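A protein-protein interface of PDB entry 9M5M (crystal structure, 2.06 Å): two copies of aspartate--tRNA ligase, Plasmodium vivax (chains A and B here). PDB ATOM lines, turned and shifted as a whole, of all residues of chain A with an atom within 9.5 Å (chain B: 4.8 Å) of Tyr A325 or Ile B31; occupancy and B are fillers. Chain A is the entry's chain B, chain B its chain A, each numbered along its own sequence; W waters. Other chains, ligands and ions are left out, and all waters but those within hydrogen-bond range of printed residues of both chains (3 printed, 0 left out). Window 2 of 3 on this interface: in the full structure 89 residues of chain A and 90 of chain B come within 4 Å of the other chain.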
ATOM      1  N   THR A 322       8.767  -6.401 -17.469  1.00  0.00           N
ATOM      2  CA  THR A 322       7.984  -7.603 -17.220  1.00  0.00           C
ATOM      3  C   THR A 322       8.897  -8.785 -16.914  1.00  0.00           C
ATOM      4  O   THR A 322      10.105  -8.763 -17.168  1.00  0.00           O
ATOM      5  CB  THR A 322       7.092  -7.949 -18.433  1.00  0.00           C
ATOM      6  OG1 THR A 322       7.900  -8.268 -19.571  1.00  0.00           O
ATOM      7  CG2 THR A 322       6.217  -6.794 -18.796  1.00  0.00           C
ATOM      8  N   TYR A 323       8.302  -9.850 -16.385  1.00  0.00           N
ATOM      9  CA  TYR A 323       8.989 -11.131 -16.279  1.00  0.00           C
ATOM     10  C   TYR A 323       8.038 -12.226 -16.761  1.00  0.00           C
ATOM     11  O   TYR A 323       6.854 -11.987 -17.024  1.00  0.00           O
ATOM     12  CB  TYR A 323       9.492 -11.398 -14.842  1.00  0.00           C
ATOM     13  CG  TYR A 323       8.411 -11.356 -13.774  1.00  0.00           C
ATOM     14  CD1 TYR A 323       7.697 -12.515 -13.422  1.00  0.00           C
ATOM     15  CD2 TYR A 323       8.131 -10.178 -13.089  1.00  0.00           C
ATOM     16  CE1 TYR A 323       6.702 -12.485 -12.438  1.00  0.00           C
ATOM     17  CE2 TYR A 323       7.149 -10.140 -12.112  1.00  0.00           C
ATOM     18  CZ  TYR A 323       6.430 -11.296 -11.794  1.00  0.00           C
ATOM     19  OH  TYR A 323       5.445 -11.244 -10.832  1.00  0.00           O
ATOM     20  N   LYS A 324       8.566 -13.439 -16.895  1.00  0.00           N
ATOM     21  CA  LYS A 324       7.788 -14.553 -17.435  1.00  0.00           C
ATOM     22  C   LYS A 324       7.008 -15.278 -16.344  1.00  0.00           C
ATOM     23  O   LYS A 324       5.771 -15.294 -16.368  1.00  0.00           O
ATOM     24  CB  LYS A 324       8.714 -15.529 -18.169  1.00  0.00           C
ATOM     25  CG  LYS A 324       9.412 -14.906 -19.365  1.00  0.00           C
ATOM     26  CD  LYS A 324      10.505 -15.827 -19.898  1.00  0.00           C
ATOM     27  CE  LYS A 324      11.093 -15.255 -21.170  1.00  0.00           C
ATOM     28  NZ  LYS A 324      12.282 -16.027 -21.640  1.00  0.00           N
ATOM     29  N   TYR A 325       7.718 -15.876 -15.375  1.00  0.00           N
ATOM     30  CA  TYR A 325       7.072 -16.673 -14.336  1.00  0.00           C
ATOM     31  C   TYR A 325       7.535 -16.314 -12.922  1.00  0.00           C
ATOM     32  O   TYR A 325       6.776 -16.492 -11.964  1.00  0.00           O
ATOM     33  CB  TYR A 325       7.296 -18.172 -14.629  1.00  0.00           C
ATOM     34  CG  TYR A 325       6.596 -18.593 -15.905  1.00  0.00           C
ATOM     35  CD1 TYR A 325       5.207 -18.683 -15.949  1.00  0.00           C
ATOM     36  CD2 TYR A 325       7.313 -18.853 -17.086  1.00  0.00           C
ATOM     37  CE1 TYR A 325       4.537 -19.031 -17.114  1.00  0.00           C
ATOM     38  CE2 TYR A 325       6.634 -19.224 -18.273  1.00  0.00           C
ATOM     39  CZ  TYR A 325       5.246 -19.310 -18.265  1.00  0.00           C
ATOM     40  OH  TYR A 325       4.524 -19.658 -19.403  1.00  0.00           O
ATOM     41  N   ASP A 326       8.750 -15.781 -12.773  1.00  0.00           N
ATOM     42  CA  ASP A 326       9.363 -15.584 -11.460  1.00  0.00           C
ATOM     43  C   ASP A 326      10.013 -14.208 -11.425  1.00  0.00           C
ATOM     44  O   ASP A 326      10.848 -13.907 -12.277  1.00  0.00           O
ATOM     45  CB  ASP A 326      10.400 -16.691 -11.208  1.00  0.00           C
ATOM     46  CG  ASP A 326      10.884 -16.750  -9.767  1.00  0.00           C
ATOM     47  OD1 ASP A 326      10.928 -15.715  -9.067  1.00  0.00           O
ATOM     48  OD2 ASP A 326      11.254 -17.866  -9.348  1.00  0.00           O
ATOM     49  N   TYR A 327       9.633 -13.366 -10.453  1.00  0.00           N
ATOM     50  CA  TYR A 327      10.219 -12.026 -10.373  1.00  0.00           C
ATOM     51  C   TYR A 327      11.740 -12.068 -10.184  1.00  0.00           C
ATOM     52  O   TYR A 327      12.428 -11.095 -10.528  1.00  0.00           O
ATOM     53  CB  TYR A 327       9.563 -11.222  -9.236  1.00  0.00           C
ATOM     54  CG  TYR A 327      10.185 -11.458  -7.861  1.00  0.00           C
ATOM     55  CD1 TYR A 327      10.995 -10.495  -7.262  1.00  0.00           C
ATOM     56  CD2 TYR A 327       9.973 -12.655  -7.171  1.00  0.00           C
ATOM     57  CE1 TYR A 327      11.568 -10.714  -6.005  1.00  0.00           C
ATOM     58  CE2 TYR A 327      10.550 -12.888  -5.916  1.00  0.00           C
ATOM     59  CZ  TYR A 327      11.347 -11.912  -5.341  1.00  0.00           C
ATOM     60  OH  TYR A 327      11.920 -12.141  -4.100  1.00  0.00           O
ATOM     61  N   LEU A 328      12.283 -13.186  -9.690  1.00  0.00           N
ATOM     62  CA  LEU A 328      13.733 -13.310  -9.553  1.00  0.00           C
ATOM     63  C   LEU A 328      14.443 -13.231 -10.902  1.00  0.00           C
ATOM     64  O   LEU A 328      15.605 -12.811 -10.951  1.00  0.00           O
ATOM     65  CB  LEU A 328      14.100 -14.616  -8.821  1.00  0.00           C
ATOM     66  CG  LEU A 328      13.712 -14.609  -7.338  1.00  0.00           C
ATOM     67  CD1 LEU A 328      13.934 -15.972  -6.675  1.00  0.00           C
ATOM     68  CD2 LEU A 328      14.491 -13.524  -6.590  1.00  0.00           C
ATOM     69  N   GLU A 329      13.767 -13.591 -12.007  1.00  0.00           N
ATOM     70  CA  GLU A 329      14.332 -13.321 -13.333  1.00  0.00           C
ATOM     71  C   GLU A 329      14.811 -11.873 -13.431  1.00  0.00           C
ATOM     72  O   GLU A 329      15.910 -11.600 -13.930  1.00  0.00           O
ATOM     73  CB  GLU A 329      13.308 -13.580 -14.446  1.00  0.00           C
ATOM     74  CG  GLU A 329      12.734 -14.990 -14.565  1.00  0.00           C
ATOM     75  CD  GLU A 329      11.395 -15.004 -15.339  1.00  0.00           C
ATOM     76  OE1 GLU A 329      11.202 -14.135 -16.236  1.00  0.00           O
ATOM     77  OE2 GLU A 329      10.533 -15.872 -15.031  1.00  0.00           O
ATOM     78  N   ASN A 330      13.978 -10.930 -12.978  1.00  0.00           N
ATOM     79  CA  ASN A 330      14.344  -9.519 -13.049  1.00  0.00           C
ATOM     80  C   ASN A 330      15.441  -9.174 -12.043  1.00  0.00           C
ATOM     81  O   ASN A 330      16.328  -8.362 -12.337  1.00  0.00           O
ATOM     82  CB  ASN A 330      13.114  -8.636 -12.806  1.00  0.00           C
ATOM     83  CG  ASN A 330      12.042  -8.782 -13.897  1.00  0.00           C
ATOM     84  OD1 ASN A 330      12.227  -9.437 -14.923  1.00  0.00           O
ATOM     85  ND2 ASN A 330      10.944  -8.123 -13.691  1.00  0.00           N
ATOM     86  N   MET A 439       4.201  -6.530  -4.122  1.00  0.00           N
ATOM     87  CA  MET A 439       3.464  -7.787  -4.006  1.00  0.00           C
ATOM     88  C   MET A 439       4.007  -8.601  -2.831  1.00  0.00           C
ATOM     89  O   MET A 439       5.219  -8.824  -2.716  1.00  0.00           O
ATOM     90  CB  MET A 439       3.529  -8.594  -5.307  1.00  0.00           C
ATOM     91  CG  MET A 439       2.668  -9.890  -5.303  1.00  0.00           C
ATOM     92  SD  MET A 439       0.945  -9.594  -4.820  1.00  0.00           S
ATOM     93  CE  MET A 439       0.389 -11.273  -4.489  1.00  0.00           C
ATOM     94  N   GLU A 442       2.031 -14.781  -1.215  1.00  0.00           N
ATOM     95  CA  GLU A 442       0.700 -15.236  -0.857  1.00  0.00           C
ATOM     96  C   GLU A 442       0.626 -16.237   0.261  1.00  0.00           C
ATOM     97  O   GLU A 442      -0.292 -16.215   1.032  1.00  0.00           O
ATOM     98  CB  GLU A 442      -0.139 -15.630  -2.074  1.00  0.00           C
ATOM     99  CG  GLU A 442      -1.263 -14.627  -2.297  1.00  0.00           C
ATOM    100  CD  GLU A 442      -1.756 -14.513  -3.728  1.00  0.00           C
ATOM    101  OE1 GLU A 442      -1.038 -14.905  -4.647  1.00  0.00           O
ATOM    102  OE2 GLU A 442      -2.870 -13.998  -3.928  1.00  0.00           O
ATOM    103  N   ASN A 449       7.955  -9.845  -1.972  1.00  0.00           N
ATOM    104  CA  ASN A 449       8.903 -10.107  -3.056  1.00  0.00           C
ATOM    105  C   ASN A 449       9.592  -8.795  -3.438  1.00  0.00           C
ATOM    106  O   ASN A 449       9.304  -8.164  -4.463  1.00  0.00           O
ATOM    107  CB  ASN A 449       8.191 -10.749  -4.234  1.00  0.00           C
ATOM    108  CG  ASN A 449       7.820 -12.192  -3.951  1.00  0.00           C
ATOM    109  OD1 ASN A 449       8.386 -12.810  -3.053  1.00  0.00           O
ATOM    110  ND2 ASN A 449       6.874 -12.736  -4.713  1.00  0.00           N
ATOM    111  N   GLN A 465       8.827  -6.865  -7.060  1.00  0.00           N
ATOM    112  CA  GLN A 465       7.672  -7.351  -7.807  1.00  0.00           C
ATOM    113  C   GLN A 465       6.467  -6.480  -7.468  1.00  0.00           C
ATOM    114  O   GLN A 465       6.225  -6.165  -6.299  1.00  0.00           O
ATOM    115  CB  GLN A 465       7.382  -8.823  -7.455  1.00  0.00           C
ATOM    116  CG  GLN A 465       6.173  -9.439  -8.195  1.00  0.00           C
ATOM    117  CD  GLN A 465       5.837 -10.864  -7.753  1.00  0.00           C
ATOM    118  OE1 GLN A 465       6.684 -11.596  -7.257  1.00  0.00           O
ATOM    119  NE2 GLN A 465       4.593 -11.261  -7.950  1.00  0.00           N
ATOM    120  N   ARG A 466       5.727  -6.065  -8.491  1.00  0.00           N
ATOM    121  CA  ARG A 466       4.578  -5.190  -8.311  1.00  0.00           C
ATOM    122  C   ARG A 466       3.314  -6.027  -8.261  1.00  0.00           C
ATOM    123  O   ARG A 466       3.220  -7.081  -8.901  1.00  0.00           O
ATOM    124  CB  ARG A 466       4.460  -4.162  -9.447  1.00  0.00           C
ATOM    125  CG  ARG A 466       5.787  -3.545  -9.899  1.00  0.00           C
ATOM    126  CD  ARG A 466       6.516  -2.819  -8.749  1.00  0.00           C
ATOM    127  NE  ARG A 466       7.595  -1.991  -9.291  1.00  0.00           N
ATOM    128  CZ  ARG A 466       8.526  -1.386  -8.566  1.00  0.00           C
ATOM    129  NH1 ARG A 466       8.586  -1.539  -7.250  1.00  0.00           N
ATOM    130  NH2 ARG A 466       9.420  -0.609  -9.177  1.00  0.00           N
ATOM    131  N   SER A 468       0.122  -6.843  -9.681  1.00  0.00           N
ATOM    132  CA  SER A 468      -0.358  -6.690 -11.050  1.00  0.00           C
ATOM    133  C   SER A 468      -1.791  -7.200 -11.202  1.00  0.00           C
ATOM    134  O   SER A 468      -2.213  -7.612 -12.285  1.00  0.00           O
ATOM    135  CB  SER A 468       0.589  -7.394 -12.020  1.00  0.00           C
ATOM    136  OG  SER A 468       0.756  -8.741 -11.627  1.00  0.00           O
ATOM    137  N   SER A 498      -2.811  -6.725 -16.775  1.00  0.00           N
ATOM    138  CA  SER A 498      -1.519  -6.253 -16.303  1.00  0.00           C
ATOM    139  C   SER A 498      -0.519  -7.397 -16.392  1.00  0.00           C
ATOM    140  O   SER A 498      -0.762  -8.470 -15.830  1.00  0.00           O
ATOM    141  CB  SER A 498      -1.636  -5.748 -14.863  1.00  0.00           C
ATOM    142  OG  SER A 498      -0.399  -5.241 -14.424  1.00  0.00           O
ATOM    143  N   TYR A 499       0.581  -7.183 -17.117  1.00  0.00           N
ATOM    144  CA  TYR A 499       1.652  -8.155 -17.160  1.00  0.00           C
ATOM    145  C   TYR A 499       2.298  -8.273 -15.788  1.00  0.00           C
ATOM    146  O   TYR A 499       2.346  -7.306 -15.026  1.00  0.00           O
ATOM    147  CB  TYR A 499       2.727  -7.753 -18.165  1.00  0.00           C
ATOM    148  CG  TYR A 499       2.245  -7.602 -19.589  1.00  0.00           C
ATOM    149  CD1 TYR A 499       2.230  -8.687 -20.456  1.00  0.00           C
ATOM    150  CD2 TYR A 499       1.830  -6.361 -20.070  1.00  0.00           C
ATOM    151  CE1 TYR A 499       1.787  -8.548 -21.770  1.00  0.00           C
ATOM    152  CE2 TYR A 499       1.387  -6.212 -21.370  1.00  0.00           C
ATOM    153  CZ  TYR A 499       1.370  -7.308 -22.217  1.00  0.00           C
ATOM    154  OH  TYR A 499       0.926  -7.145 -23.513  1.00  0.00           O
ATOM    155  N   PRO A 500       2.804  -9.449 -15.450  1.00  0.00           N
ATOM    156  CA  PRO A 500       3.673  -9.549 -14.272  1.00  0.00           C
ATOM    157  C   PRO A 500       4.918  -8.706 -14.497  1.00  0.00           C
ATOM    158  O   PRO A 500       5.559  -8.779 -15.542  1.00  0.00           O
ATOM    159  CB  PRO A 500       3.989 -11.050 -14.166  1.00  0.00           C
ATOM    160  CG  PRO A 500       3.408 -11.715 -15.398  1.00  0.00           C
ATOM    161  CD  PRO A 500       2.614 -10.720 -16.178  1.00  0.00           C
ATOM    162  N   HIS A 501       5.221  -7.846 -13.534  1.00  0.00           N
ATOM    163  CA  HIS A 501       6.327  -6.929 -13.734  1.00  0.00           C
ATOM    164  C   HIS A 501       6.960  -6.598 -12.393  1.00  0.00           C
ATOM    165  O   HIS A 501       6.414  -6.887 -11.325  1.00  0.00           O
ATOM    166  CB  HIS A 501       5.892  -5.654 -14.493  1.00  0.00           C
ATOM    167  CG  HIS A 501       4.834  -4.829 -13.810  1.00  0.00           C
ATOM    168  ND1 HIS A 501       3.498  -5.174 -13.813  1.00  0.00           N
ATOM    169  CD2 HIS A 501       4.907  -3.633 -13.170  1.00  0.00           C
ATOM    170  CE1 HIS A 501       2.798  -4.247 -13.178  1.00  0.00           C
ATOM    171  NE2 HIS A 501       3.628  -3.298 -12.784  1.00  0.00           N
ATOM    172  N   VAL B  29      -5.374 -18.936 -14.504  1.00  0.00           N
ATOM    173  CA  VAL B  29      -4.288 -19.561 -13.762  1.00  0.00           C
ATOM    174  C   VAL B  29      -3.502 -18.495 -13.027  1.00  0.00           C
ATOM    175  O   VAL B  29      -3.326 -17.374 -13.515  1.00  0.00           O
ATOM    176  CB  VAL B  29      -3.334 -20.379 -14.665  1.00  0.00           C
ATOM    177  CG1 VAL B  29      -4.028 -21.576 -15.238  1.00  0.00           C
ATOM    178  CG2 VAL B  29      -2.769 -19.512 -15.766  1.00  0.00           C
ATOM    179  N   LYS B  30      -3.025 -18.851 -11.839  1.00  0.00           N
ATOM    180  CA  LYS B  30      -1.992 -18.063 -11.192  1.00  0.00           C
ATOM    181  C   LYS B  30      -0.658 -18.367 -11.850  1.00  0.00           C
ATOM    182  O   LYS B  30      -0.425 -19.474 -12.343  1.00  0.00           O
ATOM    183  CB  LYS B  30      -1.922 -18.361  -9.693  1.00  0.00           C
ATOM    184  CG  LYS B  30      -3.144 -17.911  -8.900  1.00  0.00           C
ATOM    185  CD  LYS B  30      -2.855 -17.895  -7.403  1.00  0.00           C
ATOM    186  CE  LYS B  30      -3.242 -16.554  -6.766  1.00  0.00           C
ATOM    187  NZ  LYS B  30      -4.668 -16.514  -6.336  1.00  0.00           N
ATOM    188  N   ILE B  31       0.207 -17.351 -11.888  1.00  0.00           N
ATOM    189  CA  ILE B  31       1.550 -17.521 -12.430  1.00  0.00           C
ATOM    190  C   ILE B  31       2.293 -18.649 -11.719  1.00  0.00           C
ATOM    191  O   ILE B  31       3.073 -19.381 -12.343  1.00  0.00           O
ATOM    192  CB  ILE B  31       2.311 -16.183 -12.330  1.00  0.00           C
ATOM    193  CG1 ILE B  31       1.756 -15.185 -13.337  1.00  0.00           C
ATOM    194  CG2 ILE B  31       3.780 -16.383 -12.596  1.00  0.00           C
ATOM    195  CD1 ILE B  31       2.000 -15.605 -14.767  1.00  0.00           C
ATOM    196  N   SER B  32       2.055 -18.825 -10.435  1.00  0.00           N
ATOM    197  CA  SER B  32       2.743 -19.862  -9.693  1.00  0.00           C
ATOM    198  C   SER B  32       2.408 -21.258 -10.150  1.00  0.00           C
ATOM    199  O   SER B  32       3.195 -22.153 -10.015  1.00  0.00           O
ATOM    200  CB  SER B  32       2.478 -19.730  -8.204  1.00  0.00           C
ATOM    201  OG  SER B  32       1.120 -19.874  -7.905  1.00  0.00           O
ATOM    202  N   LYS B  33       1.241 -21.436 -10.727  1.00  0.00           N
ATOM    203  CA  LYS B  33       0.831 -22.742 -11.178  1.00  0.00           C
ATOM    204  C   LYS B  33       1.297 -23.084 -12.567  1.00  0.00           C
ATOM    205  O   LYS B  33       1.094 -24.176 -13.007  1.00  0.00           O
ATOM    206  CB  LYS B  33      -0.676 -22.885 -11.109  1.00  0.00           C
ATOM    207  CG  LYS B  33      -1.223 -22.930  -9.709  1.00  0.00           C
ATOM    208  CD  LYS B  33      -2.427 -23.845  -9.643  1.00  0.00           C
ATOM    209  CE  LYS B  33      -2.522 -24.503  -8.281  1.00  0.00           C
ATOM    210  NZ  LYS B  33      -3.449 -25.662  -8.231  1.00  0.00           N
ATOM    211  N   MET B  34       1.974 -22.190 -13.259  1.00  0.00           N
ATOM    212  CA  MET B  34       2.404 -22.500 -14.612  1.00  0.00           C
ATOM    213  C   MET B  34       3.694 -23.306 -14.666  1.00  0.00           C
ATOM    214  O   MET B  34       4.708 -22.838 -15.116  1.00  0.00           O
ATOM    215  CB  MET B  34       2.583 -21.219 -15.412  1.00  0.00           C
ATOM    216  CG  MET B  34       1.322 -20.421 -15.653  1.00  0.00           C
ATOM    217  SD  MET B  34       0.243 -21.185 -16.854  1.00  0.00           S
ATOM    218  CE  MET B  34       1.095 -20.897 -18.378  1.00  0.00           C
ATOM    219  N   ILE B  41       8.643 -23.733 -18.382  1.00  0.00           N
ATOM    220  CA  ILE B  41       8.101 -23.571 -19.727  1.00  0.00           C
ATOM    221  C   ILE B  41       9.008 -22.630 -20.510  1.00  0.00           C
ATOM    222  O   ILE B  41       9.387 -21.567 -20.007  1.00  0.00           O
ATOM    223  CB  ILE B  41       6.668 -23.016 -19.662  1.00  0.00           C
ATOM    224  CG1 ILE B  41       5.683 -24.072 -19.148  1.00  0.00           C
ATOM    225  CG2 ILE B  41       6.237 -22.461 -21.013  1.00  0.00           C
ATOM    226  CD1 ILE B  41       4.316 -23.494 -18.783  1.00  0.00           C
ATOM    227  N   LEU B  43       8.926 -19.948 -22.805  1.00  0.00           N
ATOM    228  CA  LEU B  43       7.887 -19.015 -23.218  1.00  0.00           C
ATOM    229  C   LEU B  43       8.435 -18.014 -24.231  1.00  0.00           C
ATOM    230  O   LEU B  43       9.410 -17.319 -23.945  1.00  0.00           O
ATOM    231  CB  LEU B  43       7.335 -18.276 -22.003  1.00  0.00           C
ATOM    232  CG  LEU B  43       6.199 -17.290 -22.268  1.00  0.00           C
ATOM    233  CD1 LEU B  43       4.981 -18.014 -22.865  1.00  0.00           C
ATOM    234  CD2 LEU B  43       5.838 -16.522 -20.999  1.00  0.00           C
ATOM    235  N   ARG B  93       3.001 -15.962 -25.092  1.00  0.00           N
ATOM    236  CA  ARG B  93       2.190 -15.054 -24.294  1.00  0.00           C
ATOM    237  C   ARG B  93       1.781 -13.863 -25.147  1.00  0.00           C
ATOM    238  O   ARG B  93       2.519 -13.431 -26.037  1.00  0.00           O
ATOM    239  CB  ARG B  93       2.954 -14.564 -23.050  1.00  0.00           C
ATOM    240  CG  ARG B  93       2.191 -13.553 -22.189  1.00  0.00           C
ATOM    241  CD  ARG B  93       2.827 -13.380 -20.812  1.00  0.00           C
ATOM    242  NE  ARG B  93       2.838 -14.629 -20.050  1.00  0.00           N
ATOM    243  CZ  ARG B  93       3.523 -14.813 -18.927  1.00  0.00           C
ATOM    244  NH1 ARG B  93       4.259 -13.842 -18.400  1.00  0.00           N
ATOM    245  NH2 ARG B  93       3.461 -15.994 -18.311  1.00  0.00           N
ATOM    246  N   ASP B 146      -1.455 -17.189 -21.940  1.00  0.00           N
ATOM    247  CA  ASP B 146      -0.420 -18.115 -22.368  1.00  0.00           C
ATOM    248  C   ASP B 146      -1.074 -19.217 -23.191  1.00  0.00           C
ATOM    249  O   ASP B 146      -1.990 -19.900 -22.717  1.00  0.00           O
ATOM    250  CB  ASP B 146       0.320 -18.699 -21.162  1.00  0.00           C
ATOM    251  CG  ASP B 146       1.270 -17.690 -20.509  1.00  0.00           C
ATOM    252  OD1 ASP B 146       1.311 -16.522 -20.975  1.00  0.00           O
ATOM    253  OD2 ASP B 146       1.975 -18.062 -19.534  1.00  0.00           O
ATOM    254  N   ILE B 175      -3.730 -15.465 -17.634  1.00  0.00           N
ATOM    255  CA  ILE B 175      -3.018 -15.062 -16.429  1.00  0.00           C
ATOM    256  C   ILE B 175      -3.410 -13.668 -15.949  1.00  0.00           C
ATOM    257  O   ILE B 175      -3.135 -13.333 -14.792  1.00  0.00           O
ATOM    258  CB  ILE B 175      -1.494 -15.134 -16.634  1.00  0.00           C
ATOM    259  CG1 ILE B 175      -1.066 -14.173 -17.746  1.00  0.00           C
ATOM    260  CG2 ILE B 175      -1.068 -16.578 -16.930  1.00  0.00           C
ATOM    261  CD1 ILE B 175       0.381 -13.780 -17.683  1.00  0.00           C
HETATM  262  O   HOH W   1      11.314 -18.874 -21.484  1.00  0.00           O
HETATM  263  O   HOH W   2       0.532 -17.108  -5.996  1.00  0.00           O
HETATM  264  O   HOH W   3       5.105 -11.102 -19.221  1.00  0.00           O
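The backbone carbonyl oxygen (O) of Tyr A323 is in hydrogen-bond range of the guanidinium group (NH1) of Arg B93, 3.5 Å away. The side-chain carboxylate (OE2) of Glu A442 is in salt-bridge range of the side-chain amino group (NZ) of Lys B30 (3.9 Å). O of Lys A324 lies within hydrogen-bond range of NH1 of Arg B93 (2.9 Å). The side-chain carboxylate (OD2) of Asp B146 is in hydrogen-bond range of the side-chain hydroxyl (OH) of Tyr A325, at 3.0 Å.
OE1 of Glu A329 is in hydrogen-bond range of N of Lys A324 (2.8 Å). OH of Tyr A323 sits at hydrogen-bond distance from NE2 of Gln A465 (3.0 Å). NE of Arg B93 lies within salt-bridge range of OD1 of Asp B146 (2.6 Å). N of Tyr A323 lies within hydrogen-bond range of O of Pro A500. The backbone NH (N) of Tyr A325 lies within hydrogen-bond range of the side-chain carboxylate (OE2) of Glu A329 (2.8 Å).
Lys A324 touches Leu B43 (CE to O, 3.8 Å). Tyr A325 touches Ile B31 (O to CG2, 3.1 Å). Tyr A325 touches Met B34. Tyr A325 touches Ile B41. Tyr A325 touches Leu B43. Tyr A325 touches Arg B93. Arg B93 touches Pro A500.
Of the printed residues of chain B, Tyr A323 touches Arg B93 (3.5 Å). Of chain B, only Ile B31 (3.1 Å), Met B34 (3.4 Å), Ile B41 (3.7 Å), Leu B43 (3.8 Å), Arg B93 (3.4 Å) and Asp B146 (3.0 Å) come within 4 Å of Tyr A325. Printed residues of chain B within 4 Å of Glu A442: Lys B30 (3.5 Å). Of the printed residues of chain B, Pro A500 touches Arg B93. Ile B31 touches just one residue of chain A: Tyr A325 (3.1 Å). No residue of chain A comes within 4 Å of Ser B32. Met B34 touches just one residue of chain A: Tyr A325 (3.4 Å). Ile B41 touches just one residue of chain A: Tyr A325 (3.7 Å). Printed residues of chain A within 4 Å of Leu B43: Lys A324 and Tyr A325. Printed residues of chain A within 4 Å of Asp B146: Tyr A325 (3.0 Å). The nearest printed residue of chain B that does not touch Tyr A325 is Ser B32 (5.5 Å). The nearest residue of chain A that does not touch Ile B31 is Lys A324 (4.1 Å). The nearest printed residue of chain A that does not touch Asp B146 is Lys A324 (5.7 Å).
Of the 19 printed residues of chain A, 5 touch a printed residue of chain B. Printed residues of chain A that touch a printed residue of chain B: Tyr A323, Lys A324, Tyr A325, Glu A442 and Pro A500. Hydrophobic or aromatic side chains of chain A that line the printed part of chain B: Tyr A325 and Pro A500. Of the 11 printed residues of chain B, 7 touch a printed residue of chain A. Along chain B the printed residues that touch a printed residue of chain A span positions 30 to 146. Among the printed residues, Asp or Glu carboxylates within 4 Å of a Lys or Arg side-chain nitrogen of the other chain: Glu A442 with Lys B30.
No position is printed for both chains. Of the 11 pairs that touch across the chains among the printed residues, none has its exchanged pair printed and touching as well.
Water W1 bridges the backbone NH of Leu B43 and the side-chain amino group of Lys A324. Water W3 lies within hydrogen-bond range of the backbone carbonyl oxygen of Tyr A323 (2.9 Å) and the guanidinium group of Arg B93 (3.0 Å). Water W2 lies within hydrogen-bond range of OE1 of Glu A442 and OG of Ser B32.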
